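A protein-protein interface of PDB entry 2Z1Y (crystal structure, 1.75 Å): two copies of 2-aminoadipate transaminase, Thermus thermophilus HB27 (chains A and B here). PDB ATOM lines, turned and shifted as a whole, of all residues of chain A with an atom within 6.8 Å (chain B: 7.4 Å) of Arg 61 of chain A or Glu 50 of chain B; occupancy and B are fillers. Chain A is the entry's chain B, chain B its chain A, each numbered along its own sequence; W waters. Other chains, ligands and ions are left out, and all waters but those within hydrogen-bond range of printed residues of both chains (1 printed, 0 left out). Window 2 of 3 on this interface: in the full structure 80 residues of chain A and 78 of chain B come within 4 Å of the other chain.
The side-chain carboxylate of Glu 65 of chain A lies within salt-bridge range of the side-chain amino group of Lys 49 of chain B, at 3.2 Å.
OE2 of Glu 50 of chain B lies within salt-bridge range of NH2 of Arg 61 of chain A (2.7 Å).
The backbone carbonyl oxygen (O) of Ile 59 of chain A is in hydrogen-bond range of the backbone NH (N) of Gly 64 of chain A, 3.1 Å away.
Among the printed residues, merely in contact across the chains: Leu 60 of chain A with Lys 49 of chain B (3.4 Å), Ala 57 of chain A with Ala 53 of chain B (3.5 Å), Arg 61 of chain A with Ala 53 of chain B (3.6 Å), Leu 60 of chain A with Ala 52 of chain B (3.6 Å), Leu 60 of chain A with Ala 56 of chain B (3.7 Å), Glu 65 of chain A with Phe 47 of chain B (3.8 Å), Leu 60 of chain A with Ala 53 of chain B (3.9 Å) and Gly 64 of chain A with Lys 49 of chain B (3.9 Å).
Of the printed residues of chain B, Arg 61 of chain A touches Glu 50 (2.7 Å) and Ala 53 (3.6 Å).
Of chain A, only Arg 61 comes within 4 Å of Glu 50 of chain B.
Printed residues of chain B within 4 Å of Leu 60 of chain A: Lys 49, Ala 52, Ala 53 and Ala 56.
Printed residues of chain A within 4 Å of Ala 53 of chain B: Ala 57, Leu 60 and Arg 61.
Printed residues of chain A within 4 Å of Phe 47 of chain B: Glu 65.
Ala 57 of chain B touches none of the printed residues of chain A.
The nearest residue of chain A that does not touch Glu 50 of chain B is Leu 60 of chain A (5.5 Å).
Of the 11 printed residues of chain A, 5 touch a printed residue of chain B.
Printed residues of chain A that touch a printed residue of chain B: Ala 57, Leu 60, Arg 61, Gly 64 and Glu 65.
Printed residues of chain B that touch a printed residue of chain A: Phe 47, Lys 49, Glu 50, Ala 52, Ala 53 and Ala 56.
Along chain B the printed residues that touch a printed residue of chain A span positions 47 to 56.
Among the printed residues, 10 pairs touch across the chains.
Positions printed for both chains: 54, 56 and 57.
Water W1 lies within hydrogen-bond range of O of Arg 61 of chain A, NZ of Lys 49 of chain B and O of Glu 62 of chain A.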
ATOM      1  N   GLU A  54       2.208   3.094   0.554  1.00  0.00           N
ATOM      2  CA  GLU A  54       1.893   2.282  -0.620  1.00  0.00           C
ATOM      3  C   GLU A  54       3.138   2.044  -1.469  1.00  0.00           C
ATOM      4  O   GLU A  54       3.383   0.924  -1.919  1.00  0.00           O
ATOM      5  CB  GLU A  54       0.808   2.900  -1.502  1.00  0.00           C
ATOM      6  CG  GLU A  54      -0.530   2.936  -0.754  1.00  0.00           C
ATOM      7  CD  GLU A  54      -1.785   3.508  -1.412  1.00  0.00           C
ATOM      8  OE1 GLU A  54      -2.779   3.914  -0.685  1.00  0.00           O
ATOM      9  OE2 GLU A  54      -1.741   3.512  -2.682  1.00  0.00           O
ATOM     10  N   ALA A  56       6.345   2.262  -0.542  1.00  0.00           N
ATOM     11  CA  ALA A  56       7.362   1.479   0.149  1.00  0.00           C
ATOM     12  C   ALA A  56       6.989  -0.006   0.041  1.00  0.00           C
ATOM     13  O   ALA A  56       7.860  -0.889  -0.093  1.00  0.00           O
ATOM     14  CB  ALA A  56       7.472   1.888   1.619  1.00  0.00           C
ATOM     15  N   ALA A  57       5.686  -0.296   0.194  1.00  0.00           N
ATOM     16  CA  ALA A  57       5.273  -1.695   0.226  1.00  0.00           C
ATOM     17  C   ALA A  57       5.476  -2.314  -1.152  1.00  0.00           C
ATOM     18  O   ALA A  57       5.971  -3.450  -1.267  1.00  0.00           O
ATOM     19  CB  ALA A  57       3.828  -1.806   0.627  1.00  0.00           C
ATOM     20  N   ARG A  58       5.175  -1.537  -2.192  1.00  0.00           N
ATOM     21  CA  ARG A  58       5.371  -1.976  -3.569  1.00  0.00           C
ATOM     22  C   ARG A  58       6.857  -2.169  -3.855  1.00  0.00           C
ATOM     23  O   ARG A  58       7.243  -3.198  -4.420  1.00  0.00           O
ATOM     24  CB  ARG A  58       4.699  -1.028  -4.559  1.00  0.00           C
ATOM     25  CG  ARG A  58       4.679  -1.447  -6.023  1.00  0.00           C
ATOM     26  CD  ARG A  58       4.060  -0.347  -6.940  1.00  0.00           C
ATOM     27  NE  ARG A  58       3.152   0.579  -6.229  1.00  0.00           N
ATOM     28  CZ  ARG A  58       3.322   1.900  -5.906  1.00  0.00           C
ATOM     29  NH1 ARG A  58       4.345   2.563  -6.414  1.00  0.00           N
ATOM     30  NH2 ARG A  58       2.452   2.548  -5.085  1.00  0.00           N
ATOM     31  N   ILE A  59       7.703  -1.215  -3.424  1.00  0.00           N
ATOM     32  CA  ILE A  59       9.140  -1.394  -3.608  1.00  0.00           C
ATOM     33  C   ILE A  59       9.614  -2.684  -2.963  1.00  0.00           C
ATOM     34  O   ILE A  59      10.399  -3.438  -3.527  1.00  0.00           O
ATOM     35  CB  ILE A  59       9.967  -0.203  -3.069  1.00  0.00           C
ATOM     36  CG1 ILE A  59       9.793   0.984  -3.996  1.00  0.00           C
ATOM     37  CG2 ILE A  59      11.438  -0.556  -2.956  1.00  0.00           C
ATOM     38  CD1 ILE A  59       9.959   2.328  -3.318  1.00  0.00           C
ATOM     39  N   LEU A  60       9.240  -2.914  -1.721  1.00  0.00           N
ATOM     40  CA  LEU A  60       9.813  -4.062  -1.051  1.00  0.00           C
ATOM     41  C   LEU A  60       9.266  -5.373  -1.632  1.00  0.00           C
ATOM     42  O   LEU A  60      10.007  -6.349  -1.731  1.00  0.00           O
ATOM     43  CB  LEU A  60       9.517  -3.872   0.422  1.00  0.00           C
ATOM     44  CG  LEU A  60      10.399  -2.835   1.112  1.00  0.00           C
ATOM     45  CD1 LEU A  60       9.849  -2.329   2.415  1.00  0.00           C
ATOM     46  CD2 LEU A  60      11.799  -3.323   1.276  1.00  0.00           C
ATOM     47  N   ARG A  61       8.011  -5.414  -2.086  1.00  0.00           N
ATOM     48  CA  ARG A  61       7.506  -6.661  -2.636  1.00  0.00           C
ATOM     49  C   ARG A  61       8.028  -6.950  -4.035  1.00  0.00           C
ATOM     50  O   ARG A  61       8.314  -8.127  -4.310  1.00  0.00           O
ATOM     51  CB  ARG A  61       5.975  -6.614  -2.758  1.00  0.00           C
ATOM     52  CG  ARG A  61       5.322  -6.677  -1.389  1.00  0.00           C
ATOM     53  CD  ARG A  61       3.813  -6.456  -1.507  1.00  0.00           C
ATOM     54  NE  ARG A  61       3.217  -6.838  -0.224  1.00  0.00           N
ATOM     55  CZ  ARG A  61       2.473  -6.056   0.539  1.00  0.00           C
ATOM     56  NH1 ARG A  61       2.003  -4.956   0.006  1.00  0.00           N
ATOM     57  NH2 ARG A  61       2.024  -6.500   1.701  1.00  0.00           N
ATOM     58  N   GLU A  62       8.090  -5.928  -4.898  1.00  0.00           N
ATOM     59  CA  GLU A  62       8.439  -6.103  -6.303  1.00  0.00           C
ATOM     60  C   GLU A  62       9.939  -6.023  -6.560  1.00  0.00           C
ATOM     61  O   GLU A  62      10.463  -6.579  -7.539  1.00  0.00           O
ATOM     62  CB  GLU A  62       7.685  -5.055  -7.110  1.00  0.00           C
ATOM     63  CG  GLU A  62       6.170  -5.198  -6.943  1.00  0.00           C
ATOM     64  CD  GLU A  62       5.313  -4.265  -7.811  1.00  0.00           C
ATOM     65  OE1 GLU A  62       4.070  -4.233  -7.523  1.00  0.00           O
ATOM     66  OE2 GLU A  62       5.839  -3.536  -8.717  1.00  0.00           O
ATOM     67  N   LYS A  63      10.649  -5.257  -5.729  1.00  0.00           N
ATOM     68  CA  LYS A  63      12.057  -4.971  -5.980  1.00  0.00           C
ATOM     69  C   LYS A  63      12.858  -5.070  -4.697  1.00  0.00           C
ATOM     70  O   LYS A  63      13.939  -4.471  -4.559  1.00  0.00           O
ATOM     71  CB  LYS A  63      12.165  -3.529  -6.477  1.00  0.00           C
ATOM     72  CG  LYS A  63      11.615  -3.340  -7.875  1.00  0.00           C
ATOM     73  CD  LYS A  63      11.799  -1.939  -8.424  1.00  0.00           C
ATOM     74  CE  LYS A  63      11.064  -1.722  -9.722  1.00  0.00           C
ATOM     75  NZ  LYS A  63      11.171  -0.341 -10.241  1.00  0.00           N
ATOM     76  N   GLY A  64      12.349  -5.849  -3.745  1.00  0.00           N
ATOM     77  CA  GLY A  64      12.996  -5.897  -2.452  1.00  0.00           C
ATOM     78  C   GLY A  64      14.413  -6.473  -2.493  1.00  0.00           C
ATOM     79  O   GLY A  64      15.241  -6.170  -1.633  1.00  0.00           O
ATOM     80  N   GLU A  65      14.695  -7.395  -3.445  1.00  0.00           N
ATOM     81  CA  GLU A  65      16.055  -7.937  -3.596  1.00  0.00           C
ATOM     82  C   GLU A  65      17.063  -6.854  -3.996  1.00  0.00           C
ATOM     83  O   GLU A  65      18.226  -7.036  -3.688  1.00  0.00           O
ATOM     84  CB  GLU A  65      16.118  -9.157  -4.517  1.00  0.00           C
ATOM     85  CG  GLU A  65      15.282 -10.293  -3.970  1.00  0.00           C
ATOM     86  CD  GLU A  65      15.357 -11.629  -4.709  1.00  0.00           C
ATOM     87  OE1 GLU A  65      14.244 -12.165  -4.924  1.00  0.00           O
ATOM     88  OE2 GLU A  65      16.446 -12.132  -5.070  1.00  0.00           O
ATOM     89  N   PHE B  47      16.150 -12.320   2.552  1.00  0.00           N
ATOM     90  CA  PHE B  47      15.523 -11.037   2.829  1.00  0.00           C
ATOM     91  C   PHE B  47      14.028 -11.264   3.070  1.00  0.00           C
ATOM     92  O   PHE B  47      13.377 -11.907   2.251  1.00  0.00           O
ATOM     93  CB  PHE B  47      15.682 -10.118   1.645  1.00  0.00           C
ATOM     94  CG  PHE B  47      17.075  -9.634   1.294  1.00  0.00           C
ATOM     95  CD1 PHE B  47      18.113  -9.600   2.226  1.00  0.00           C
ATOM     96  CD2 PHE B  47      17.305  -9.205   0.018  1.00  0.00           C
ATOM     97  CE1 PHE B  47      19.377  -9.185   1.852  1.00  0.00           C
ATOM     98  CE2 PHE B  47      18.554  -8.727  -0.337  1.00  0.00           C
ATOM     99  CZ  PHE B  47      19.563  -8.720   0.582  1.00  0.00           C
ATOM    100  N   PRO B  48      13.428 -10.713   4.137  1.00  0.00           N
ATOM    101  CA  PRO B  48      11.988 -10.899   4.370  1.00  0.00           C
ATOM    102  C   PRO B  48      11.216  -9.803   3.630  1.00  0.00           C
ATOM    103  O   PRO B  48      10.751  -8.847   4.259  1.00  0.00           O
ATOM    104  CB  PRO B  48      11.946 -10.752   5.856  1.00  0.00           C
ATOM    105  CG  PRO B  48      12.954  -9.716   6.155  1.00  0.00           C
ATOM    106  CD  PRO B  48      14.094  -9.924   5.187  1.00  0.00           C
ATOM    107  N   LYS B  49      11.129  -9.917   2.310  1.00  0.00           N
ATOM    108  CA  LYS B  49      10.466  -8.900   1.495  1.00  0.00           C
ATOM    109  C   LYS B  49       9.029  -8.685   1.979  1.00  0.00           C
ATOM    110  O   LYS B  49       8.608  -7.538   2.168  1.00  0.00           O
ATOM    111  CB  LYS B  49      10.553  -9.271   0.016  1.00  0.00           C
ATOM    112  CG  LYS B  49      11.971  -9.305  -0.536  1.00  0.00           C
ATOM    113  CD  LYS B  49      12.012  -9.643  -2.018  1.00  0.00           C
ATOM    114  CE  LYS B  49      11.506 -11.052  -2.235  1.00  0.00           C
ATOM    115  NZ  LYS B  49      11.421 -11.247  -3.676  1.00  0.00           N
ATOM    116  N   GLU B  50       8.256  -9.744   2.169  1.00  0.00           N
ATOM    117  CA  GLU B  50       6.818  -9.515   2.368  1.00  0.00           C
ATOM    118  C   GLU B  50       6.580  -8.905   3.752  1.00  0.00           C
ATOM    119  O   GLU B  50       5.822  -7.943   3.930  1.00  0.00           O
ATOM    120  CB  GLU B  50       5.995 -10.791   2.124  1.00  0.00           C
ATOM    121  CG  GLU B  50       4.561 -10.609   2.633  1.00  0.00           C
ATOM    122  CD  GLU B  50       3.762  -9.579   1.873  1.00  0.00           C
ATOM    123  OE1 GLU B  50       4.135  -9.305   0.716  1.00  0.00           O
ATOM    124  OE2 GLU B  50       2.786  -8.999   2.467  1.00  0.00           O
ATOM    125  N   GLU B  51       7.245  -9.438   4.773  1.00  0.00           N
ATOM    126  CA  GLU B  51       7.201  -8.907   6.131  1.00  0.00           C
ATOM    127  C   GLU B  51       7.712  -7.459   6.154  1.00  0.00           C
ATOM    128  O   GLU B  51       7.148  -6.655   6.865  1.00  0.00           O
ATOM    129  CB  GLU B  51       8.006  -9.747   7.124  1.00  0.00           C
ATOM    130  CG  GLU B  51       7.702  -9.511   8.604  1.00  0.00           C
ATOM    131  CD  GLU B  51       8.487 -10.297   9.654  1.00  0.00           C
ATOM    132  OE1 GLU B  51       9.101 -11.282   9.159  1.00  0.00           O
ATOM    133  OE2 GLU B  51       8.607  -9.906  10.872  1.00  0.00           O
ATOM    134  N   ALA B  52       8.790  -7.182   5.420  1.00  0.00           N
ATOM    135  CA  ALA B  52       9.300  -5.808   5.372  1.00  0.00           C
ATOM    136  C   ALA B  52       8.265  -4.836   4.784  1.00  0.00           C
ATOM    137  O   ALA B  52       8.066  -3.713   5.263  1.00  0.00           O
ATOM    138  CB  ALA B  52      10.595  -5.751   4.624  1.00  0.00           C
ATOM    139  N   ALA B  53       7.600  -5.278   3.719  1.00  0.00           N
ATOM    140  CA  ALA B  53       6.610  -4.464   3.028  1.00  0.00           C
ATOM    141  C   ALA B  53       5.451  -4.099   3.953  1.00  0.00           C
ATOM    142  O   ALA B  53       5.072  -2.931   4.026  1.00  0.00           O
ATOM    143  CB  ALA B  53       6.124  -5.164   1.783  1.00  0.00           C
ATOM    144  N   GLU B  54       4.954  -5.104   4.682  1.00  0.00           N
ATOM    145  CA  GLU B  54       3.874  -4.915   5.640  1.00  0.00           C
ATOM    146  C   GLU B  54       4.284  -3.946   6.733  1.00  0.00           C
ATOM    147  O   GLU B  54       3.527  -3.037   7.100  1.00  0.00           O
ATOM    148  CB  GLU B  54       3.428  -6.211   6.322  1.00  0.00           C
ATOM    149  CG  GLU B  54       2.234  -5.986   7.246  1.00  0.00           C
ATOM    150  CD  GLU B  54       2.466  -5.632   8.704  1.00  0.00           C
ATOM    151  OE1 GLU B  54       1.423  -5.345   9.313  1.00  0.00           O
ATOM    152  OE2 GLU B  54       3.581  -5.654   9.281  1.00  0.00           O
ATOM    153  N   ALA B  55       5.484  -4.159   7.267  1.00  0.00           N
ATOM    154  CA  ALA B  55       5.972  -3.377   8.375  1.00  0.00           C
ATOM    155  C   ALA B  55       6.260  -1.935   7.989  1.00  0.00           C
ATOM    156  O   ALA B  55       5.898  -1.030   8.735  1.00  0.00           O
ATOM    157  CB  ALA B  55       7.212  -4.031   9.005  1.00  0.00           C
ATOM    158  N   ALA B  56       6.868  -1.718   6.820  1.00  0.00           N
ATOM    159  CA  ALA B  56       7.166  -0.375   6.339  1.00  0.00           C
ATOM    160  C   ALA B  56       5.871   0.396   6.059  1.00  0.00           C
ATOM    161  O   ALA B  56       5.734   1.566   6.429  1.00  0.00           O
ATOM    162  CB  ALA B  56       7.978  -0.474   5.057  1.00  0.00           C
ATOM    163  N   ALA B  57       4.871  -0.292   5.464  1.00  0.00           N
ATOM    164  CA  ALA B  57       3.606   0.410   5.230  1.00  0.00           C
ATOM    165  C   ALA B  57       2.936   0.795   6.550  1.00  0.00           C
ATOM    166  O   ALA B  57       2.421   1.900   6.665  1.00  0.00           O
ATOM    167  CB  ALA B  57       2.688  -0.395   4.388  1.00  0.00           C
ATOM    168  N   LEU B 281      10.958  -5.720  12.421  1.00  0.00           N
ATOM    169  CA  LEU B 281      11.300  -7.031  11.919  1.00  0.00           C
ATOM    170  C   LEU B 281      11.899  -7.983  12.940  1.00  0.00           C
ATOM    171  O   LEU B 281      11.737  -9.221  12.814  1.00  0.00           O
ATOM    172  CB  LEU B 281      12.159  -6.862  10.661  1.00  0.00           C
ATOM    173  CG  LEU B 281      11.427  -6.361   9.420  1.00  0.00           C
ATOM    174  CD1 LEU B 281      12.403  -6.015   8.320  1.00  0.00           C
ATOM    175  CD2 LEU B 281      10.382  -7.328   8.896  1.00  0.00           C
HETATM  176  O   HOH W   1      10.633  -9.144  -5.515  1.00  0.00           O
